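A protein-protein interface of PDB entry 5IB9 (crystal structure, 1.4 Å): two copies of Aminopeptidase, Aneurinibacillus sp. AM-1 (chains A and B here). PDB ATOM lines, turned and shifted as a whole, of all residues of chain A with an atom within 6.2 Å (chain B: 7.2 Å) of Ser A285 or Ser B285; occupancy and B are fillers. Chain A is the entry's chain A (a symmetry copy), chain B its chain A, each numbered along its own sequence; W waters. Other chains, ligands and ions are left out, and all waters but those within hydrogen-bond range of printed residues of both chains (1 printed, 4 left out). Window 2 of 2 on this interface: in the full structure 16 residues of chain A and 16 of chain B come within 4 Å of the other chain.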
ATOM      1  N   GLN A  58      35.382   6.064  25.077  1.00  0.00           N
ATOM      2  CA  GLN A  58      34.049   6.526  25.544  1.00  0.00           C
ATOM      3  C   GLN A  58      33.855   8.009  25.199  1.00  0.00           C
ATOM      4  O   GLN A  58      34.572   8.824  25.726  1.00  0.00           O
ATOM      5  CB  GLN A  58      33.914   6.271  27.045  1.00  0.00           C
ATOM      6  CG  GLN A  58      32.500   6.750  27.599  1.00  0.00           C
ATOM      7  CD  GLN A  58      32.474   6.846  29.067  1.00  0.00           C
ATOM      8  OE1 GLN A  58      33.509   6.889  29.787  1.00  0.00           O
ATOM      9  NE2 GLN A  58      31.301   6.842  29.628  1.00  0.00           N
ATOM     10  N   LYS A 280      34.023  11.817  35.636  1.00  0.00           N
ATOM     11  CA  LYS A 280      32.612  11.712  36.106  1.00  0.00           C
ATOM     12  C   LYS A 280      31.836  10.851  35.106  1.00  0.00           C
ATOM     13  O   LYS A 280      31.007  10.015  35.563  1.00  0.00           O
ATOM     14  CB  LYS A 280      31.985  13.126  36.097  1.00  0.00           C
ATOM     15  CG  LYS A 280      32.408  13.895  37.368  1.00  0.00           C
ATOM     16  CD  LYS A 280      31.875  15.370  37.253  1.00  0.00           C
ATOM     17  CE  LYS A 280      32.382  16.169  38.487  1.00  0.00           C
ATOM     18  NZ  LYS A 280      31.977  17.641  38.362  1.00  0.00           N
ATOM     19  N   LYS A 281      32.037  11.031  33.796  1.00  0.00           N
ATOM     20  CA  LYS A 281      31.315  10.212  32.807  1.00  0.00           C
ATOM     21  C   LYS A 281      31.801   8.811  32.894  1.00  0.00           C
ATOM     22  O   LYS A 281      30.979   7.913  32.701  1.00  0.00           O
ATOM     23  CB  LYS A 281      31.464  10.770  31.381  1.00  0.00           C
ATOM     24  CG  LYS A 281      30.868  12.165  31.206  1.00  0.00           C
ATOM     25  CD  LYS A 281      29.337  12.140  31.061  1.00  0.00           C
ATOM     26  CE  LYS A 281      28.925  13.640  30.819  1.00  0.00           C
ATOM     27  NZ  LYS A 281      27.439  13.762  30.914  1.00  0.00           N
ATOM     28  N   TYR A 282      33.061   8.528  33.158  1.00  0.00           N
ATOM     29  CA  TYR A 282      33.467   7.117  33.236  1.00  0.00           C
ATOM     30  C   TYR A 282      32.912   6.444  34.529  1.00  0.00           C
ATOM     31  O   TYR A 282      32.379   5.352  34.488  1.00  0.00           O
ATOM     32  CB  TYR A 282      34.987   6.985  33.177  1.00  0.00           C
ATOM     33  CG  TYR A 282      35.369   5.509  33.254  1.00  0.00           C
ATOM     34  CD1 TYR A 282      35.244   4.679  32.104  1.00  0.00           C
ATOM     35  CD2 TYR A 282      35.793   4.947  34.445  1.00  0.00           C
ATOM     36  CE1 TYR A 282      35.446   3.346  32.212  1.00  0.00           C
ATOM     37  CE2 TYR A 282      35.988   3.616  34.590  1.00  0.00           C
ATOM     38  CZ  TYR A 282      35.837   2.862  33.430  1.00  0.00           C
ATOM     39  OH  TYR A 282      36.039   1.447  33.516  1.00  0.00           O
ATOM     40  N   ALA A 283      33.046   7.091  35.680  1.00  0.00           N
ATOM     41  CA  ALA A 283      32.447   6.611  36.945  1.00  0.00           C
ATOM     42  C   ALA A 283      30.975   6.353  36.757  1.00  0.00           C
ATOM     43  O   ALA A 283      30.515   5.322  37.270  1.00  0.00           O
ATOM     44  CB  ALA A 283      32.697   7.708  38.003  1.00  0.00           C
ATOM     45  N   ALA A 284      30.284   7.201  35.998  1.00  0.00           N
ATOM     46  CA  ALA A 284      28.805   6.941  35.816  1.00  0.00           C
ATOM     47  C   ALA A 284      28.553   5.741  34.951  1.00  0.00           C
ATOM     48  O   ALA A 284      27.358   5.256  34.935  1.00  0.00           O
ATOM     49  CB  ALA A 284      28.166   8.139  35.192  1.00  0.00           C
ATOM     50  N   SER A 285      29.525   5.200  34.256  1.00  0.00           N
ATOM     51  CA  SER A 285      29.285   3.968  33.456  1.00  0.00           C
ATOM     52  C   SER A 285      29.389   2.669  34.257  1.00  0.00           C
ATOM     53  O   SER A 285      29.105   1.585  33.674  1.00  0.00           O
ATOM     54  CB  SER A 285      30.287   3.905  32.268  1.00  0.00           C
ATOM     55  OG  SER A 285      31.584   3.485  32.715  1.00  0.00           O
ATOM     56  N   LEU A 286      29.937   2.706  35.448  1.00  0.00           N
ATOM     57  CA  LEU A 286      30.171   1.507  36.244  1.00  0.00           C
ATOM     58  C   LEU A 286      28.896   0.890  36.819  1.00  0.00           C
ATOM     59  O   LEU A 286      28.011   1.640  37.268  1.00  0.00           O
ATOM     60  CB  LEU A 286      31.135   1.828  37.400  1.00  0.00           C
ATOM     61  CG  LEU A 286      32.512   2.373  36.914  1.00  0.00           C
ATOM     62  CD1 LEU A 286      33.366   2.746  38.119  1.00  0.00           C
ATOM     63  CD2 LEU A 286      33.185   1.240  35.997  1.00  0.00           C
ATOM     64  N   SER A 287      28.857  -0.447  36.831  1.00  0.00           N
ATOM     65  CA  SER A 287      27.746  -1.078  37.542  1.00  0.00           C
ATOM     66  C   SER A 287      28.026  -1.139  39.000  1.00  0.00           C
ATOM     67  O   SER A 287      29.165  -0.905  39.472  1.00  0.00           O
ATOM     68  CB  SER A 287      27.606  -2.463  37.024  1.00  0.00           C
ATOM     69  OG  SER A 287      28.716  -3.316  37.425  1.00  0.00           O
ATOM     70  N   GLU A 290      30.787  -3.673  39.599  1.00  0.00           N
ATOM     71  CA  GLU A 290      32.128  -3.067  39.320  1.00  0.00           C
ATOM     72  C   GLU A 290      32.537  -2.156  40.406  1.00  0.00           C
ATOM     73  O   GLU A 290      33.724  -2.249  40.819  1.00  0.00           O
ATOM     74  CB  GLU A 290      32.073  -2.338  37.983  1.00  0.00           C
ATOM     75  CG  GLU A 290      31.960  -3.336  36.788  1.00  0.00           C
ATOM     76  CD  GLU A 290      31.816  -2.547  35.526  1.00  0.00           C
ATOM     77  OE1 GLU A 290      30.896  -1.714  35.333  1.00  0.00           O
ATOM     78  OE2 GLU A 290      32.652  -2.656  34.611  1.00  0.00           O
ATOM     79  N   GLN B  58      23.154  -0.944  36.750  1.00  0.00           N
ATOM     80  CA  GLN B  58      23.812   0.385  36.652  1.00  0.00           C
ATOM     81  C   GLN B  58      23.061   1.410  37.513  1.00  0.00           C
ATOM     82  O   GLN B  58      21.928   1.698  37.213  1.00  0.00           O
ATOM     83  CB  GLN B  58      23.880   0.816  35.188  1.00  0.00           C
ATOM     84  CG  GLN B  58      24.578   2.239  35.024  1.00  0.00           C
ATOM     85  CD  GLN B  58      24.345   2.831  33.698  1.00  0.00           C
ATOM     86  OE1 GLN B  58      23.437   2.452  32.909  1.00  0.00           O
ATOM     87  NE2 GLN B  58      25.166   3.770  33.329  1.00  0.00           N
ATOM     88  N   PRO B  59      23.702   1.982  38.558  1.00  0.00           N
ATOM     89  CA  PRO B  59      23.005   2.973  39.424  1.00  0.00           C
ATOM     90  C   PRO B  59      23.138   4.295  38.792  1.00  0.00           C
ATOM     91  O   PRO B  59      24.142   4.561  38.060  1.00  0.00           O
ATOM     92  CB  PRO B  59      23.792   2.910  40.758  1.00  0.00           C
ATOM     93  CG  PRO B  59      25.265   2.621  40.281  1.00  0.00           C
ATOM     94  CD  PRO B  59      25.113   1.730  39.004  1.00  0.00           C
ATOM     95  N   ILE B 207      20.744  -4.770  33.227  1.00  0.00           N
ATOM     96  CA  ILE B 207      21.257  -5.064  31.880  1.00  0.00           C
ATOM     97  C   ILE B 207      21.692  -6.555  31.804  1.00  0.00           C
ATOM     98  O   ILE B 207      22.548  -7.004  32.587  1.00  0.00           O
ATOM     99  CB  ILE B 207      22.479  -4.236  31.546  1.00  0.00           C
ATOM    100  CG1 ILE B 207      22.153  -2.746  31.595  1.00  0.00           C
ATOM    101  CG2 ILE B 207      23.040  -4.599  30.120  1.00  0.00           C
ATOM    102  CD1 ILE B 207      23.058  -2.031  32.543  1.00  0.00           C
ATOM    103  N   ARG B 265      21.395  -7.394  24.097  1.00  0.00           N
ATOM    104  CA  ARG B 265      21.370  -6.790  25.430  1.00  0.00           C
ATOM    105  C   ARG B 265      19.934  -6.537  25.761  1.00  0.00           C
ATOM    106  O   ARG B 265      19.288  -5.690  25.066  1.00  0.00           O
ATOM    107  CB  ARG B 265      22.166  -5.459  25.446  1.00  0.00           C
ATOM    108  CG  ARG B 265      23.670  -5.677  25.014  1.00  0.00           C
ATOM    109  CD  ARG B 265      24.435  -4.403  25.107  1.00  0.00           C
ATOM    110  NE  ARG B 265      25.814  -4.715  24.745  1.00  0.00           N
ATOM    111  CZ  ARG B 265      26.756  -3.789  24.824  1.00  0.00           C
ATOM    112  NH1 ARG B 265      26.567  -2.530  25.288  1.00  0.00           N
ATOM    113  NH2 ARG B 265      27.947  -4.173  24.492  1.00  0.00           N
ATOM    114  N   SER B 279      17.674   5.551  30.483  1.00  0.00           N
ATOM    115  CA  SER B 279      18.277   5.285  29.185  1.00  0.00           C
ATOM    116  C   SER B 279      19.293   6.282  28.724  1.00  0.00           C
ATOM    117  O   SER B 279      20.241   5.937  28.034  1.00  0.00           O
ATOM    118  CB  SER B 279      17.218   5.095  28.121  1.00  0.00           C
ATOM    119  OG  SER B 279      16.339   6.235  28.044  1.00  0.00           O
ATOM    120  N   LYS B 280      19.145   7.551  29.122  1.00  0.00           N
ATOM    121  CA  LYS B 280      20.223   8.540  28.834  1.00  0.00           C
ATOM    122  C   LYS B 280      21.491   8.093  29.565  1.00  0.00           C
ATOM    123  O   LYS B 280      22.594   8.204  28.958  1.00  0.00           O
ATOM    124  CB  LYS B 280      19.800   9.910  29.415  1.00  0.00           C
ATOM    125  CG  LYS B 280      18.824  10.611  28.446  1.00  0.00           C
ATOM    126  CD  LYS B 280      18.305  11.927  29.135  1.00  0.00           C
ATOM    127  CE  LYS B 280      17.250  12.583  28.200  1.00  0.00           C
ATOM    128  NZ  LYS B 280      16.638  13.812  28.881  1.00  0.00           N
ATOM    129  N   LYS B 281      21.396   7.634  30.818  1.00  0.00           N
ATOM    130  CA  LYS B 281      22.595   7.186  31.545  1.00  0.00           C
ATOM    131  C   LYS B 281      23.105   5.942  30.915  1.00  0.00           C
ATOM    132  O   LYS B 281      24.327   5.779  30.890  1.00  0.00           O
ATOM    133  CB  LYS B 281      22.313   6.980  33.044  1.00  0.00           C
ATOM    134  CG  LYS B 281      21.902   8.260  33.769  1.00  0.00           C
ATOM    135  CD  LYS B 281      23.101   9.167  34.095  1.00  0.00           C
ATOM    136  CE  LYS B 281      22.491  10.378  34.895  1.00  0.00           C
ATOM    137  NZ  LYS B 281      23.530  11.440  35.043  1.00  0.00           N
ATOM    138  N   TYR B 282      22.293   5.037  30.406  1.00  0.00           N
ATOM    139  CA  TYR B 282      22.872   3.833  29.791  1.00  0.00           C
ATOM    140  C   TYR B 282      23.553   4.172  28.429  1.00  0.00           C
ATOM    141  O   TYR B 282      24.658   3.745  28.157  1.00  0.00           O
ATOM    142  CB  TYR B 282      21.808   2.754  29.601  1.00  0.00           C
ATOM    143  CG  TYR B 282      22.447   1.521  28.966  1.00  0.00           C
ATOM    144  CD1 TYR B 282      23.220   0.630  29.763  1.00  0.00           C
ATOM    145  CD2 TYR B 282      22.327   1.278  27.610  1.00  0.00           C
ATOM    146  CE1 TYR B 282      23.901  -0.379  29.173  1.00  0.00           C
ATOM    147  CE2 TYR B 282      23.006   0.288  26.988  1.00  0.00           C
ATOM    148  CZ  TYR B 282      23.753  -0.538  27.823  1.00  0.00           C
ATOM    149  OH  TYR B 282      24.488  -1.612  27.225  1.00  0.00           O
ATOM    150  N   ALA B 283      22.889   4.932  27.568  1.00  0.00           N
ATOM    151  CA  ALA B 283      23.484   5.422  26.304  1.00  0.00           C
ATOM    152  C   ALA B 283      24.792   6.115  26.582  1.00  0.00           C
ATOM    153  O   ALA B 283      25.730   5.876  25.808  1.00  0.00           O
ATOM    154  CB  ALA B 283      22.457   6.386  25.671  1.00  0.00           C
ATOM    155  N   ALA B 284      24.877   6.876  27.672  1.00  0.00           N
ATOM    156  CA  ALA B 284      26.191   7.575  27.944  1.00  0.00           C
ATOM    157  C   ALA B 284      27.259   6.608  28.364  1.00  0.00           C
ATOM    158  O   ALA B 284      28.478   7.029  28.366  1.00  0.00           O
ATOM    159  CB  ALA B 284      25.996   8.590  29.023  1.00  0.00           C
ATOM    160  N   SER B 285      26.956   5.376  28.693  1.00  0.00           N
ATOM    161  CA  SER B 285      28.026   4.402  29.040  1.00  0.00           C
ATOM    162  C   SER B 285      28.668   3.719  27.831  1.00  0.00           C
ATOM    163  O   SER B 285      29.651   2.951  28.034  1.00  0.00           O
ATOM    164  CB  SER B 285      27.460   3.309  29.990  1.00  0.00           C
ATOM    165  OG  SER B 285      26.683   2.349  29.260  1.00  0.00           O
ATOM    166  N   LEU B 286      28.073   3.809  26.667  1.00  0.00           N
ATOM    167  CA  LEU B 286      28.553   3.111  25.480  1.00  0.00           C
ATOM    168  C   LEU B 286      29.840   3.697  24.899  1.00  0.00           C
ATOM    169  O   LEU B 286      29.978   4.933  24.858  1.00  0.00           O
ATOM    170  CB  LEU B 286      27.465   3.120  24.393  1.00  0.00           C
ATOM    171  CG  LEU B 286      26.135   2.451  24.853  1.00  0.00           C
ATOM    172  CD1 LEU B 286      25.091   2.583  23.752  1.00  0.00           C
ATOM    173  CD2 LEU B 286      26.465   0.923  25.223  1.00  0.00           C
ATOM    174  N   SER B 287      30.719   2.805  24.429  1.00  0.00           N
ATOM    175  CA  SER B 287      31.873   3.324  23.695  1.00  0.00           C
ATOM    176  C   SER B 287      31.508   3.611  22.284  1.00  0.00           C
ATOM    177  O   SER B 287      30.431   3.210  21.777  1.00  0.00           O
ATOM    178  CB  SER B 287      32.928   2.279  23.713  1.00  0.00           C
ATOM    179  OG  SER B 287      32.574   1.124  22.899  1.00  0.00           O
ATOM    180  N   GLU B 288      32.420   4.323  21.567  1.00  0.00           N
ATOM    181  CA  GLU B 288      32.176   4.610  20.166  1.00  0.00           C
ATOM    182  C   GLU B 288      32.055   3.309  19.344  1.00  0.00           C
ATOM    183  O   GLU B 288      31.232   3.263  18.415  1.00  0.00           O
ATOM    184  CB  GLU B 288      33.285   5.560  19.594  1.00  0.00           C
ATOM    185  CG  GLU B 288      33.086   6.957  20.152  1.00  0.00           C
ATOM    186  CD  GLU B 288      34.002   8.075  19.544  1.00  0.00           C
ATOM    187  OE1 GLU B 288      34.968   7.728  18.864  1.00  0.00           O
ATOM    188  OE2 GLU B 288      33.570   9.245  19.624  1.00  0.00           O
ATOM    189  N   GLU B 290      30.943   0.316  20.485  1.00  0.00           N
ATOM    190  CA  GLU B 290      29.575  -0.217  20.780  1.00  0.00           C
ATOM    191  C   GLU B 290      28.542   0.528  20.034  1.00  0.00           C
ATOM    192  O   GLU B 290      27.644  -0.148  19.463  1.00  0.00           O
ATOM    193  CB  GLU B 290      29.327  -0.143  22.282  1.00  0.00           C
ATOM    194  CG  GLU B 290      30.204  -1.174  23.059  1.00  0.00           C
ATOM    195  CD  GLU B 290      29.976  -0.978  24.524  1.00  0.00           C
ATOM    196  OE1 GLU B 290      30.171   0.115  25.113  1.00  0.00           O
ATOM    197  OE2 GLU B 290      29.530  -1.902  25.227  1.00  0.00           O
ATOM    198  N   ILE B 291      28.601   1.869  19.955  1.00  0.00           N
ATOM    199  CA  ILE B 291      27.585   2.582  19.247  1.00  0.00           C
ATOM    200  C   ILE B 291      27.584   2.186  17.749  1.00  0.00           C
ATOM    201  O   ILE B 291      26.484   1.927  17.136  1.00  0.00           O
ATOM    202  CB  ILE B 291      27.832   4.080  19.382  1.00  0.00           C
ATOM    203  CG1 ILE B 291      27.560   4.472  20.851  1.00  0.00           C
ATOM    204  CG2 ILE B 291      26.883   4.942  18.450  1.00  0.00           C
ATOM    205  CD1 ILE B 291      28.068   5.862  21.235  1.00  0.00           C
ATOM    206  N   LEU B 354      22.041   8.908  19.582  1.00  0.00           N
ATOM    207  CA  LEU B 354      23.397   8.463  19.207  1.00  0.00           C
ATOM    208  C   LEU B 354      23.557   8.038  17.763  1.00  0.00           C
ATOM    209  O   LEU B 354      24.646   7.581  17.416  1.00  0.00           O
ATOM    210  CB  LEU B 354      23.779   7.325  20.148  1.00  0.00           C
ATOM    211  CG  LEU B 354      23.966   7.686  21.624  1.00  0.00           C
ATOM    212  CD1 LEU B 354      24.489   6.400  22.266  1.00  0.00           C
ATOM    213  CD2 LEU B 354      25.001   8.801  21.787  1.00  0.00           C
HETATM  214  O   HOH W   1      25.267   6.326  36.417  1.00  0.00           O
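The side-chain amide nitrogen of Gln B58 is in hydrogen-bond range of the backbone carbonyl oxygen of Ala A284 (3.1 Å).
O of Ala B284 sits at hydrogen-bond distance from NE2 of Gln A58, 3.1 Å away.
NE2 of Gln B58 sits at hydrogen-bond distance from O of Lys B281 (3.3 Å).
The backbone carbonyl oxygen (O) of Tyr B282 sits at hydrogen-bond distance from the side-chain hydroxyl (OG) of Ser B285 (2.7 Å).
NE2 of Gln A58 sits at hydrogen-bond distance from O of Lys A281 (3.3 Å).
The backbone carbonyl oxygen (O) of Tyr A282 is in hydrogen-bond range of the side-chain hydroxyl (OG) of Ser A285 (2.7 Å).
Ser A285 touches Ser B285 (CB to CB, 3.7 Å).
Pro B59 touches Leu A286 (CD to O, 3.4 Å).
Of the printed residues of chain B, Ala A284 touches Gln B58.
Of chain B, only Ser B285 (3.7 Å) comes within 4 Å of Ser A285.
Of the printed residues of chain B, Leu A286 touches Pro B59 (3.4 Å).
Of the printed residues of chain A, Pro B59 touches Leu A286.
Ala B283 touches none of the printed residues of chain A.
Ser B285 touches one residue of chain A.
Leu B286 touches none of the printed residues of chain A.
The nearest printed residue of chain B that does not touch Gln A58 is Ser B285 (4.1 Å).
Along chain A the printed residues that touch a printed residue of chain B span positions 58 to 286.
Among the printed residues, no Asp or Glu carboxylate lies within 4 Å of a Lys or Arg side-chain nitrogen of the other chain.
Gln A58 touches Ala B284, and with the chains exchanged Ala A284 touches Gln B58.
Ser A285 touches its own counterpart, Ser B285.
10 positions are printed for both chains.
Of the 4 pairs that touch across the chains among the printed residues, 3 have their exchanged pair printed and touching as well.
Water W1 bridges O of Pro B59 (2.7 Å) and O of Ala A284 (2.8 Å).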
